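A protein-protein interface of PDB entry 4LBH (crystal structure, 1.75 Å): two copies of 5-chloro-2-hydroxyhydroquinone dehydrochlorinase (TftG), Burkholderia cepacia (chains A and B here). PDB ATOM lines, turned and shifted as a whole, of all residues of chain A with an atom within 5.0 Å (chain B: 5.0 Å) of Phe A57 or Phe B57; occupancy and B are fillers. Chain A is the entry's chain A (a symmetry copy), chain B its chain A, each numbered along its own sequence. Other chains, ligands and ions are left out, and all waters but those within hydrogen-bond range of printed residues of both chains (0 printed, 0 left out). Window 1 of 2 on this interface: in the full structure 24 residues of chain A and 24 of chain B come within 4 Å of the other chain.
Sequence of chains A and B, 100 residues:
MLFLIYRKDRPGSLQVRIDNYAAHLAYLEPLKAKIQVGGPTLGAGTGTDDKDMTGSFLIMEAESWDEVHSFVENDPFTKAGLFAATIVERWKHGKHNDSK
NE1 of Trp B91 lies within hydrogen-bond range of O of Gly A39 (3.0 Å). The indole nitrogen (NE1) of Trp A91 is in hydrogen-bond range of the backbone carbonyl oxygen (O) of Gly B39 (3.0 Å).
The backbone NH of Phe A57 lies within hydrogen-bond range of the backbone carbonyl oxygen of Gly A39. The backbone NH (N) of Phe B57 sits at hydrogen-bond distance from the backbone carbonyl oxygen (O) of Gly B39, at 2.9 Å. OG1 of Thr A41 sits at hydrogen-bond distance from N of Gly A55, at 2.9 Å. The backbone NH of Ile A59 sits at hydrogen-bond distance from the backbone carbonyl oxygen of Val A37 (2.9 Å). The backbone carbonyl oxygen (O) of Val B37 sits at hydrogen-bond distance from the backbone NH (N) of Ile B59. The backbone NH (N) of Gly B55 sits at hydrogen-bond distance from the side-chain hydroxyl (OG1) of Thr B41.
Leu A4 touches Thr B41 (CD1 to CG2, 3.9 Å). CD1 of Leu A4 touches CG of Phe B57 (3.6 Å). Trp B91 touches Val A37 (CH2 to CG1, 3.6 Å). Pro A40 touches Trp B91. Thr A41 touches Leu B4. Phe A57 touches Phe B57 (CZ to CZ, 3.1 Å). CB of Phe A57 touches NE1 of Trp B91 (3.7 Å). Val B37 touches Ile A59. Trp A91 touches Val B37 (CH2 to CG1, 3.6 Å). CZ2 of Trp A91 touches C of Gly B38, 3.7 Å away.
Of the printed residues of chain B, Gly A38 touches Trp B91 (3.7 Å). Printed residues of chain B within 4 Å of Thr A41: Leu B4 and Trp B91. Phe A57 touches three residues of chain B. Printed residues of chain B within 4 Å of Trp A91: Val B37, Gly B38, Gly B39, Pro B40, Thr B41 and Phe B57. Ile B5 touches none of the printed residues of chain A. Of the printed residues of chain A, Gly B39 touches Trp A91. Of the printed residues of chain A, Thr B41 touches Leu A4 and Trp A91. Of chain A, only Leu A4 (3.6 Å), Phe A57 (3.1 Å) and Trp A91 (3.7 Å) come within 4 Å of Phe B57. The nearest residue of chain B that does not touch Phe A57 is Ile B59 (4.3 Å).
Of the 14 printed residues of chain A, 9 touch a printed residue of chain B. Hydrophobic or aromatic side chains of chain A within 4 Å of the printed part of chain B: Leu A4, Val A37, Phe A57, Ile A59 and Trp A91. Printed residues of chain B that touch a printed residue of chain A: Leu B4, Val B37, Gly B38, Gly B39, Pro B40, Thr B41, Phe B57, Ile B59 and Trp B91. Hydrophobic or aromatic side chains of chain B within 4 Å of the printed part of chain A: Leu B4, Val B37, Phe B57, Ile B59 and Trp B91. Among the printed residues, 19 pairs touch across the chains. Among the printed residues, no Asp or Glu carboxylate lies within 4 Å of a Lys or Arg side-chain nitrogen of the other chain.
Leu A4 touches Thr B41, and with the chains exchanged Thr A41 touches Leu B4. Val A37 touches Trp B91, and with the chains exchanged Trp A91 touches Val B37. Gly A38 touches Trp B91, and with the chains exchanged Trp A91 touches Gly B38. Phe A57 touches Trp B91, and with the chains exchanged Trp A91 touches Phe B57. Of the 19 pairs that touch across the chains among the printed residues, 19 have their exchanged pair printed and touching as well.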
ATOM      1  N   LEU A   4      23.033  15.961   9.649  1.00  0.00           N
ATOM      2  CA  LEU A   4      22.530  16.936  10.609  1.00  0.00           C
ATOM      3  C   LEU A   4      21.717  17.952   9.832  1.00  0.00           C
ATOM      4  O   LEU A   4      22.142  18.404   8.770  1.00  0.00           O
ATOM      5  CB  LEU A   4      23.685  17.669  11.304  1.00  0.00           C
ATOM      6  CG  LEU A   4      24.788  16.844  11.951  1.00  0.00           C
ATOM      7  CD1 LEU A   4      25.816  17.785  12.592  1.00  0.00           C
ATOM      8  CD2 LEU A   4      24.192  15.908  12.992  1.00  0.00           C
ATOM      9  N   ILE A   5      20.535  18.304  10.336  1.00  0.00           N
ATOM     10  CA  ILE A   5      19.730  19.325   9.679  1.00  0.00           C
ATOM     11  C   ILE A   5      19.314  20.341  10.744  1.00  0.00           C
ATOM     12  O   ILE A   5      18.508  20.030  11.613  1.00  0.00           O
ATOM     13  CB  ILE A   5      18.477  18.729   9.023  1.00  0.00           C
ATOM     14  CG1 ILE A   5      18.873  17.681   7.974  1.00  0.00           C
ATOM     15  CG2 ILE A   5      17.630  19.826   8.382  1.00  0.00           C
ATOM     16  CD1 ILE A   5      17.698  16.957   7.384  1.00  0.00           C
ATOM     17  N   TYR A   6      19.900  21.531  10.669  1.00  0.00           N
ATOM     18  CA  TYR A   6      19.745  22.585  11.684  1.00  0.00           C
ATOM     19  C   TYR A   6      19.025  23.742  11.023  1.00  0.00           C
ATOM     20  O   TYR A   6      19.443  24.225   9.979  1.00  0.00           O
ATOM     21  CB  TYR A   6      21.136  23.016  12.166  1.00  0.00           C
ATOM     22  CG  TYR A   6      21.183  24.346  12.905  1.00  0.00           C
ATOM     23  CD1 TYR A   6      21.422  25.536  12.219  1.00  0.00           C
ATOM     24  CD2 TYR A   6      21.017  24.405  14.278  1.00  0.00           C
ATOM     25  CE1 TYR A   6      21.490  26.752  12.885  1.00  0.00           C
ATOM     26  CE2 TYR A   6      21.074  25.624  14.958  1.00  0.00           C
ATOM     27  CZ  TYR A   6      21.306  26.792  14.250  1.00  0.00           C
ATOM     28  OH  TYR A   6      21.373  28.007  14.913  1.00  0.00           O
ATOM     29  N   VAL A  37      17.311  11.420  15.839  1.00  0.00           N
ATOM     30  CA  VAL A  37      17.245  12.361  16.960  1.00  0.00           C
ATOM     31  C   VAL A  37      16.548  13.597  16.434  1.00  0.00           C
ATOM     32  O   VAL A  37      16.764  13.987  15.294  1.00  0.00           O
ATOM     33  CB  VAL A  37      18.681  12.761  17.414  1.00  0.00           C
ATOM     34  CG1 VAL A  37      18.634  13.886  18.433  1.00  0.00           C
ATOM     35  CG2 VAL A  37      19.432  11.561  17.973  1.00  0.00           C
ATOM     36  N   GLY A  38      15.680  14.227  17.220  1.00  0.00           N
ATOM     37  CA  GLY A  38      15.021  15.398  16.687  1.00  0.00           C
ATOM     38  C   GLY A  38      14.307  16.178  17.767  1.00  0.00           C
ATOM     39  O   GLY A  38      13.824  15.589  18.727  1.00  0.00           O
ATOM     40  N   GLY A  39      14.236  17.493  17.594  1.00  0.00           N
ATOM     41  CA  GLY A  39      13.566  18.344  18.562  1.00  0.00           C
ATOM     42  C   GLY A  39      13.845  19.805  18.299  1.00  0.00           C
ATOM     43  O   GLY A  39      14.684  20.148  17.465  1.00  0.00           O
ATOM     44  N   PRO A  40      13.133  20.686  19.005  1.00  0.00           N
ATOM     45  CA  PRO A  40      13.304  22.130  18.825  1.00  0.00           C
ATOM     46  C   PRO A  40      14.527  22.678  19.558  1.00  0.00           C
ATOM     47  O   PRO A  40      14.874  22.228  20.666  1.00  0.00           O
ATOM     48  CB  PRO A  40      12.017  22.706  19.445  1.00  0.00           C
ATOM     49  CG  PRO A  40      11.690  21.729  20.540  1.00  0.00           C
ATOM     50  CD  PRO A  40      12.087  20.360  19.992  1.00  0.00           C
ATOM     51  N   THR A  41      15.184  23.664  18.955  1.00  0.00           N
ATOM     52  CA  THR A  41      16.096  24.490  19.723  1.00  0.00           C
ATOM     53  C   THR A  41      15.250  25.424  20.603  1.00  0.00           C
ATOM     54  O   THR A  41      14.081  25.709  20.300  1.00  0.00           O
ATOM     55  CB  THR A  41      17.026  25.315  18.832  1.00  0.00           C
ATOM     56  OG1 THR A  41      16.233  26.109  17.943  1.00  0.00           O
ATOM     57  CG2 THR A  41      17.913  24.373  17.998  1.00  0.00           C
ATOM     58  N   GLY A  55      13.691  27.038  16.782  1.00  0.00           N
ATOM     59  CA  GLY A  55      14.252  26.387  15.598  1.00  0.00           C
ATOM     60  C   GLY A  55      14.069  24.880  15.662  1.00  0.00           C
ATOM     61  O   GLY A  55      13.452  24.370  16.592  1.00  0.00           O
ATOM     62  N   SER A  56      14.620  24.163  14.680  1.00  0.00           N
ATOM     63  CA  SER A  56      14.398  22.732  14.572  1.00  0.00           C
ATOM     64  C   SER A  56      15.734  22.068  14.324  1.00  0.00           C
ATOM     65  O   SER A  56      16.509  22.560  13.518  1.00  0.00           O
ATOM     66  CB  SER A  56      13.480  22.426  13.379  1.00  0.00           C
ATOM     67  OG  SER A  56      12.160  22.933  13.577  1.00  0.00           O
ATOM     68  N   PHE A  57      16.005  20.970  15.022  1.00  0.00           N
ATOM     69  CA  PHE A  57      17.201  20.190  14.734  1.00  0.00           C
ATOM     70  C   PHE A  57      16.882  18.700  14.606  1.00  0.00           C
ATOM     71  O   PHE A  57      16.154  18.139  15.431  1.00  0.00           O
ATOM     72  CB  PHE A  57      18.262  20.410  15.811  1.00  0.00           C
ATOM     73  CG  PHE A  57      19.445  19.519  15.636  1.00  0.00           C
ATOM     74  CD1 PHE A  57      20.413  19.836  14.704  1.00  0.00           C
ATOM     75  CD2 PHE A  57      19.563  18.337  16.356  1.00  0.00           C
ATOM     76  CE1 PHE A  57      21.502  19.001  14.510  1.00  0.00           C
ATOM     77  CE2 PHE A  57      20.660  17.493  16.155  1.00  0.00           C
ATOM     78  CZ  PHE A  57      21.610  17.831  15.234  1.00  0.00           C
ATOM     79  N   LEU A  58      17.441  18.052  13.580  1.00  0.00           N
ATOM     80  CA  LEU A  58      17.162  16.646  13.326  1.00  0.00           C
ATOM     81  C   LEU A  58      18.452  15.976  12.868  1.00  0.00           C
ATOM     82  O   LEU A  58      19.301  16.617  12.248  1.00  0.00           O
ATOM     83  CB  LEU A  58      16.141  16.482  12.185  1.00  0.00           C
ATOM     84  CG  LEU A  58      14.650  16.747  12.320  1.00  0.00           C
ATOM     85  CD1 LEU A  58      14.007  16.619  10.963  1.00  0.00           C
ATOM     86  CD2 LEU A  58      14.035  15.757  13.270  1.00  0.00           C
ATOM     87  N   ILE A  59      18.591  14.694  13.188  1.00  0.00           N
ATOM     88  CA  ILE A  59      19.588  13.839  12.538  1.00  0.00           C
ATOM     89  C   ILE A  59      18.816  12.757  11.797  1.00  0.00           C
ATOM     90  O   ILE A  59      18.062  12.007  12.415  1.00  0.00           O
ATOM     91  CB  ILE A  59      20.533  13.168  13.556  1.00  0.00           C
ATOM     92  CG1 ILE A  59      21.280  14.213  14.385  1.00  0.00           C
ATOM     93  CG2 ILE A  59      21.534  12.243  12.833  1.00  0.00           C
ATOM     94  CD1 ILE A  59      22.115  13.622  15.545  1.00  0.00           C
ATOM     95  N   TRP A  91      27.279  13.391   8.498  1.00  0.00           N
ATOM     96  CA  TRP A  91      27.737  13.172   9.870  1.00  0.00           C
ATOM     97  C   TRP A  91      27.738  11.688  10.224  1.00  0.00           C
ATOM     98  O   TRP A  91      27.021  10.907   9.607  1.00  0.00           O
ATOM     99  CB  TRP A  91      26.815  13.959  10.836  1.00  0.00           C
ATOM    100  CG  TRP A  91      27.099  13.792  12.326  1.00  0.00           C
ATOM    101  CD1 TRP A  91      27.986  14.508  13.094  1.00  0.00           C
ATOM    102  CD2 TRP A  91      26.440  12.885  13.225  1.00  0.00           C
ATOM    103  NE1 TRP A  91      27.940  14.073  14.403  1.00  0.00           N
ATOM    104  CE2 TRP A  91      26.992  13.090  14.509  1.00  0.00           C
ATOM    105  CE3 TRP A  91      25.439  11.918  13.064  1.00  0.00           C
ATOM    106  CZ2 TRP A  91      26.587  12.353  15.623  1.00  0.00           C
ATOM    107  CZ3 TRP A  91      25.036  11.189  14.169  1.00  0.00           C
ATOM    108  CH2 TRP A  91      25.610  11.413  15.433  1.00  0.00           C
ATOM    109  N   LEU B   4      23.126  21.807  21.905  1.00  0.00           N
ATOM    110  CA  LEU B   4      23.789  21.405  20.670  1.00  0.00           C
ATOM    111  C   LEU B   4      25.098  22.163  20.597  1.00  0.00           C
ATOM    112  O   LEU B   4      25.135  23.363  20.867  1.00  0.00           O
ATOM    113  CB  LEU B   4      22.942  21.778  19.446  1.00  0.00           C
ATOM    114  CG  LEU B   4      21.486  21.339  19.404  1.00  0.00           C
ATOM    115  CD1 LEU B   4      20.852  21.807  18.088  1.00  0.00           C
ATOM    116  CD2 LEU B   4      21.397  19.826  19.536  1.00  0.00           C
ATOM    117  N   ILE B   5      26.186  21.475  20.254  1.00  0.00           N
ATOM    118  CA  ILE B   5      27.466  22.152  20.098  1.00  0.00           C
ATOM    119  C   ILE B   5      28.048  21.731  18.747  1.00  0.00           C
ATOM    120  O   ILE B   5      28.446  20.586  18.577  1.00  0.00           O
ATOM    121  CB  ILE B   5      28.449  21.781  21.216  1.00  0.00           C
ATOM    122  CG1 ILE B   5      27.867  22.165  22.584  1.00  0.00           C
ATOM    123  CG2 ILE B   5      29.795  22.469  21.002  1.00  0.00           C
ATOM    124  CD1 ILE B   5      28.712  21.712  23.738  1.00  0.00           C
ATOM    125  N   TYR B   6      28.057  22.667  17.804  1.00  0.00           N
ATOM    126  CA  TYR B   6      28.437  22.415  16.405  1.00  0.00           C
ATOM    127  C   TYR B   6      29.701  23.204  16.133  1.00  0.00           C
ATOM    128  O   TYR B   6      29.754  24.403  16.371  1.00  0.00           O
ATOM    129  CB  TYR B   6      27.298  22.886  15.491  1.00  0.00           C
ATOM    130  CG  TYR B   6      27.673  23.067  14.027  1.00  0.00           C
ATOM    131  CD1 TYR B   6      28.113  24.302  13.551  1.00  0.00           C
ATOM    132  CD2 TYR B   6      27.564  22.022  13.127  1.00  0.00           C
ATOM    133  CE1 TYR B   6      28.438  24.487  12.214  1.00  0.00           C
ATOM    134  CE2 TYR B   6      27.896  22.193  11.781  1.00  0.00           C
ATOM    135  CZ  TYR B   6      28.336  23.429  11.336  1.00  0.00           C
ATOM    136  OH  TYR B   6      28.662  23.615  10.003  1.00  0.00           O
ATOM    137  N   VAL B  37      24.950  12.421  22.388  1.00  0.00           N
ATOM    138  CA  VAL B  37      25.181  12.069  20.984  1.00  0.00           C
ATOM    139  C   VAL B  37      26.432  12.810  20.563  1.00  0.00           C
ATOM    140  O   VAL B  37      26.642  13.944  20.973  1.00  0.00           O
ATOM    141  CB  VAL B  37      23.996  12.562  20.102  1.00  0.00           C
ATOM    142  CG1 VAL B  37      24.309  12.391  18.627  1.00  0.00           C
ATOM    143  CG2 VAL B  37      22.706  11.839  20.465  1.00  0.00           C
ATOM    144  N   GLY B  38      27.304  12.196  19.770  1.00  0.00           N
ATOM    145  CA  GLY B  38      28.494  12.924  19.392  1.00  0.00           C
ATOM    146  C   GLY B  38      29.235  12.240  18.266  1.00  0.00           C
ATOM    147  O   GLY B  38      29.211  11.018  18.174  1.00  0.00           O
ATOM    148  N   GLY B  39      29.896  13.033  17.430  1.00  0.00           N
ATOM    149  CA  GLY B  39      30.652  12.487  16.315  1.00  0.00           C
ATOM    150  C   GLY B  39      31.085  13.573  15.358  1.00  0.00           C
ATOM    151  O   GLY B  39      30.664  14.724  15.476  1.00  0.00           O
ATOM    152  N   PRO B  40      31.944  13.217  14.400  1.00  0.00           N
ATOM    153  CA  PRO B  40      32.449  14.186  13.424  1.00  0.00           C
ATOM    154  C   PRO B  40      31.455  14.462  12.296  1.00  0.00           C
ATOM    155  O   PRO B  40      30.730  13.561  11.836  1.00  0.00           O
ATOM    156  CB  PRO B  40      33.701  13.486  12.864  1.00  0.00           C
ATOM    157  CG  PRO B  40      33.344  12.026  12.936  1.00  0.00           C
ATOM    158  CD  PRO B  40      32.522  11.873  14.214  1.00  0.00           C
ATOM    159  N   THR B  41      31.423  15.707  11.830  1.00  0.00           N
ATOM    160  CA  THR B  41      30.815  15.972  10.540  1.00  0.00           C
ATOM    161  C   THR B  41      31.780  15.459   9.459  1.00  0.00           C
ATOM    162  O   THR B  41      32.993  15.331   9.686  1.00  0.00           O
ATOM    163  CB  THR B  41      30.533  17.458  10.323  1.00  0.00           C
ATOM    164  OG1 THR B  41      31.753  18.191  10.481  1.00  0.00           O
ATOM    165  CG2 THR B  41      29.520  17.951  11.373  1.00  0.00           C
ATOM    166  N   GLY B  55      34.626  18.446  11.074  1.00  0.00           N
ATOM    167  CA  GLY B  55      34.097  19.209  12.205  1.00  0.00           C
ATOM    168  C   GLY B  55      33.598  18.287  13.305  1.00  0.00           C
ATOM    169  O   GLY B  55      33.734  17.070  13.202  1.00  0.00           O
ATOM    170  N   SER B  56      33.008  18.862  14.355  1.00  0.00           N
ATOM    171  CA  SER B  56      32.614  18.089  15.518  1.00  0.00           C
ATOM    172  C   SER B  56      31.205  18.491  15.892  1.00  0.00           C
ATOM    173  O   SER B  56      30.899  19.673  15.896  1.00  0.00           O
ATOM    174  CB  SER B  56      33.536  18.408  16.706  1.00  0.00           C
ATOM    175  OG  SER B  56      34.875  17.967  16.476  1.00  0.00           O
ATOM    176  N   PHE B  57      30.353  17.515  16.188  1.00  0.00           N
ATOM    177  CA  PHE B  57      29.026  17.824  16.701  1.00  0.00           C
ATOM    178  C   PHE B  57      28.696  16.993  17.942  1.00  0.00           C
ATOM    179  O   PHE B  57      28.927  15.780  17.967  1.00  0.00           O
ATOM    180  CB  PHE B  57      27.965  17.605  15.624  1.00  0.00           C
ATOM    181  CG  PHE B  57      26.579  17.768  16.148  1.00  0.00           C
ATOM    182  CD1 PHE B  57      26.053  19.034  16.322  1.00  0.00           C
ATOM    183  CD2 PHE B  57      25.822  16.666  16.522  1.00  0.00           C
ATOM    184  CE1 PHE B  57      24.777  19.199  16.837  1.00  0.00           C
ATOM    185  CE2 PHE B  57      24.536  16.835  17.047  1.00  0.00           C
ATOM    186  CZ  PHE B  57      24.033  18.096  17.202  1.00  0.00           C
ATOM    187  N   LEU B  58      28.137  17.640  18.968  1.00  0.00           N
ATOM    188  CA  LEU B  58      27.833  16.963  20.220  1.00  0.00           C
ATOM    189  C   LEU B  58      26.504  17.497  20.743  1.00  0.00           C
ATOM    190  O   LEU B  58      26.158  18.653  20.502  1.00  0.00           O
ATOM    191  CB  LEU B  58      28.895  17.276  21.290  1.00  0.00           C
ATOM    192  CG  LEU B  58      30.293  16.679  21.314  1.00  0.00           C
ATOM    193  CD1 LEU B  58      31.083  17.331  22.420  1.00  0.00           C
ATOM    194  CD2 LEU B  58      30.216  15.196  21.549  1.00  0.00           C
ATOM    195  N   ILE B  59      25.768  16.643  21.446  1.00  0.00           N
ATOM    196  CA  ILE B  59      24.658  17.093  22.291  1.00  0.00           C
ATOM    197  C   ILE B  59      25.026  16.734  23.722  1.00  0.00           C
ATOM    198  O   ILE B  59      25.243  15.561  24.026  1.00  0.00           O
ATOM    199  CB  ILE B  59      23.329  16.397  21.928  1.00  0.00           C
ATOM    200  CG1 ILE B  59      22.950  16.662  20.471  1.00  0.00           C
ATOM    201  CG2 ILE B  59      22.201  16.865  22.870  1.00  0.00           C
ATOM    202  CD1 ILE B  59      21.724  15.857  19.981  1.00  0.00           C
ATOM    203  N   TRP B  91      18.524  23.107  23.664  1.00  0.00           N
ATOM    204  CA  TRP B  91      17.746  22.182  22.840  1.00  0.00           C
ATOM    205  C   TRP B  91      17.038  21.138  23.698  1.00  0.00           C
ATOM    206  O   TRP B  91      17.460  20.870  24.817  1.00  0.00           O
ATOM    207  CB  TRP B  91      18.696  21.496  21.826  1.00  0.00           C
ATOM    208  CG  TRP B  91      18.070  20.438  20.922  1.00  0.00           C
ATOM    209  CD1 TRP B  91      17.437  20.633  19.718  1.00  0.00           C
ATOM    210  CD2 TRP B  91      18.077  19.017  21.139  1.00  0.00           C
ATOM    211  NE1 TRP B  91      17.023  19.424  19.197  1.00  0.00           N
ATOM    212  CE2 TRP B  91      17.415  18.421  20.043  1.00  0.00           C
ATOM    213  CE3 TRP B  91      18.578  18.195  22.158  1.00  0.00           C
ATOM    214  CZ2 TRP B  91      17.228  17.042  19.943  1.00  0.00           C
ATOM    215  CZ3 TRP B  91      18.394  16.827  22.057  1.00  0.00           C
ATOM    216  CH2 TRP B  91      17.725  16.264  20.955  1.00  0.00           C
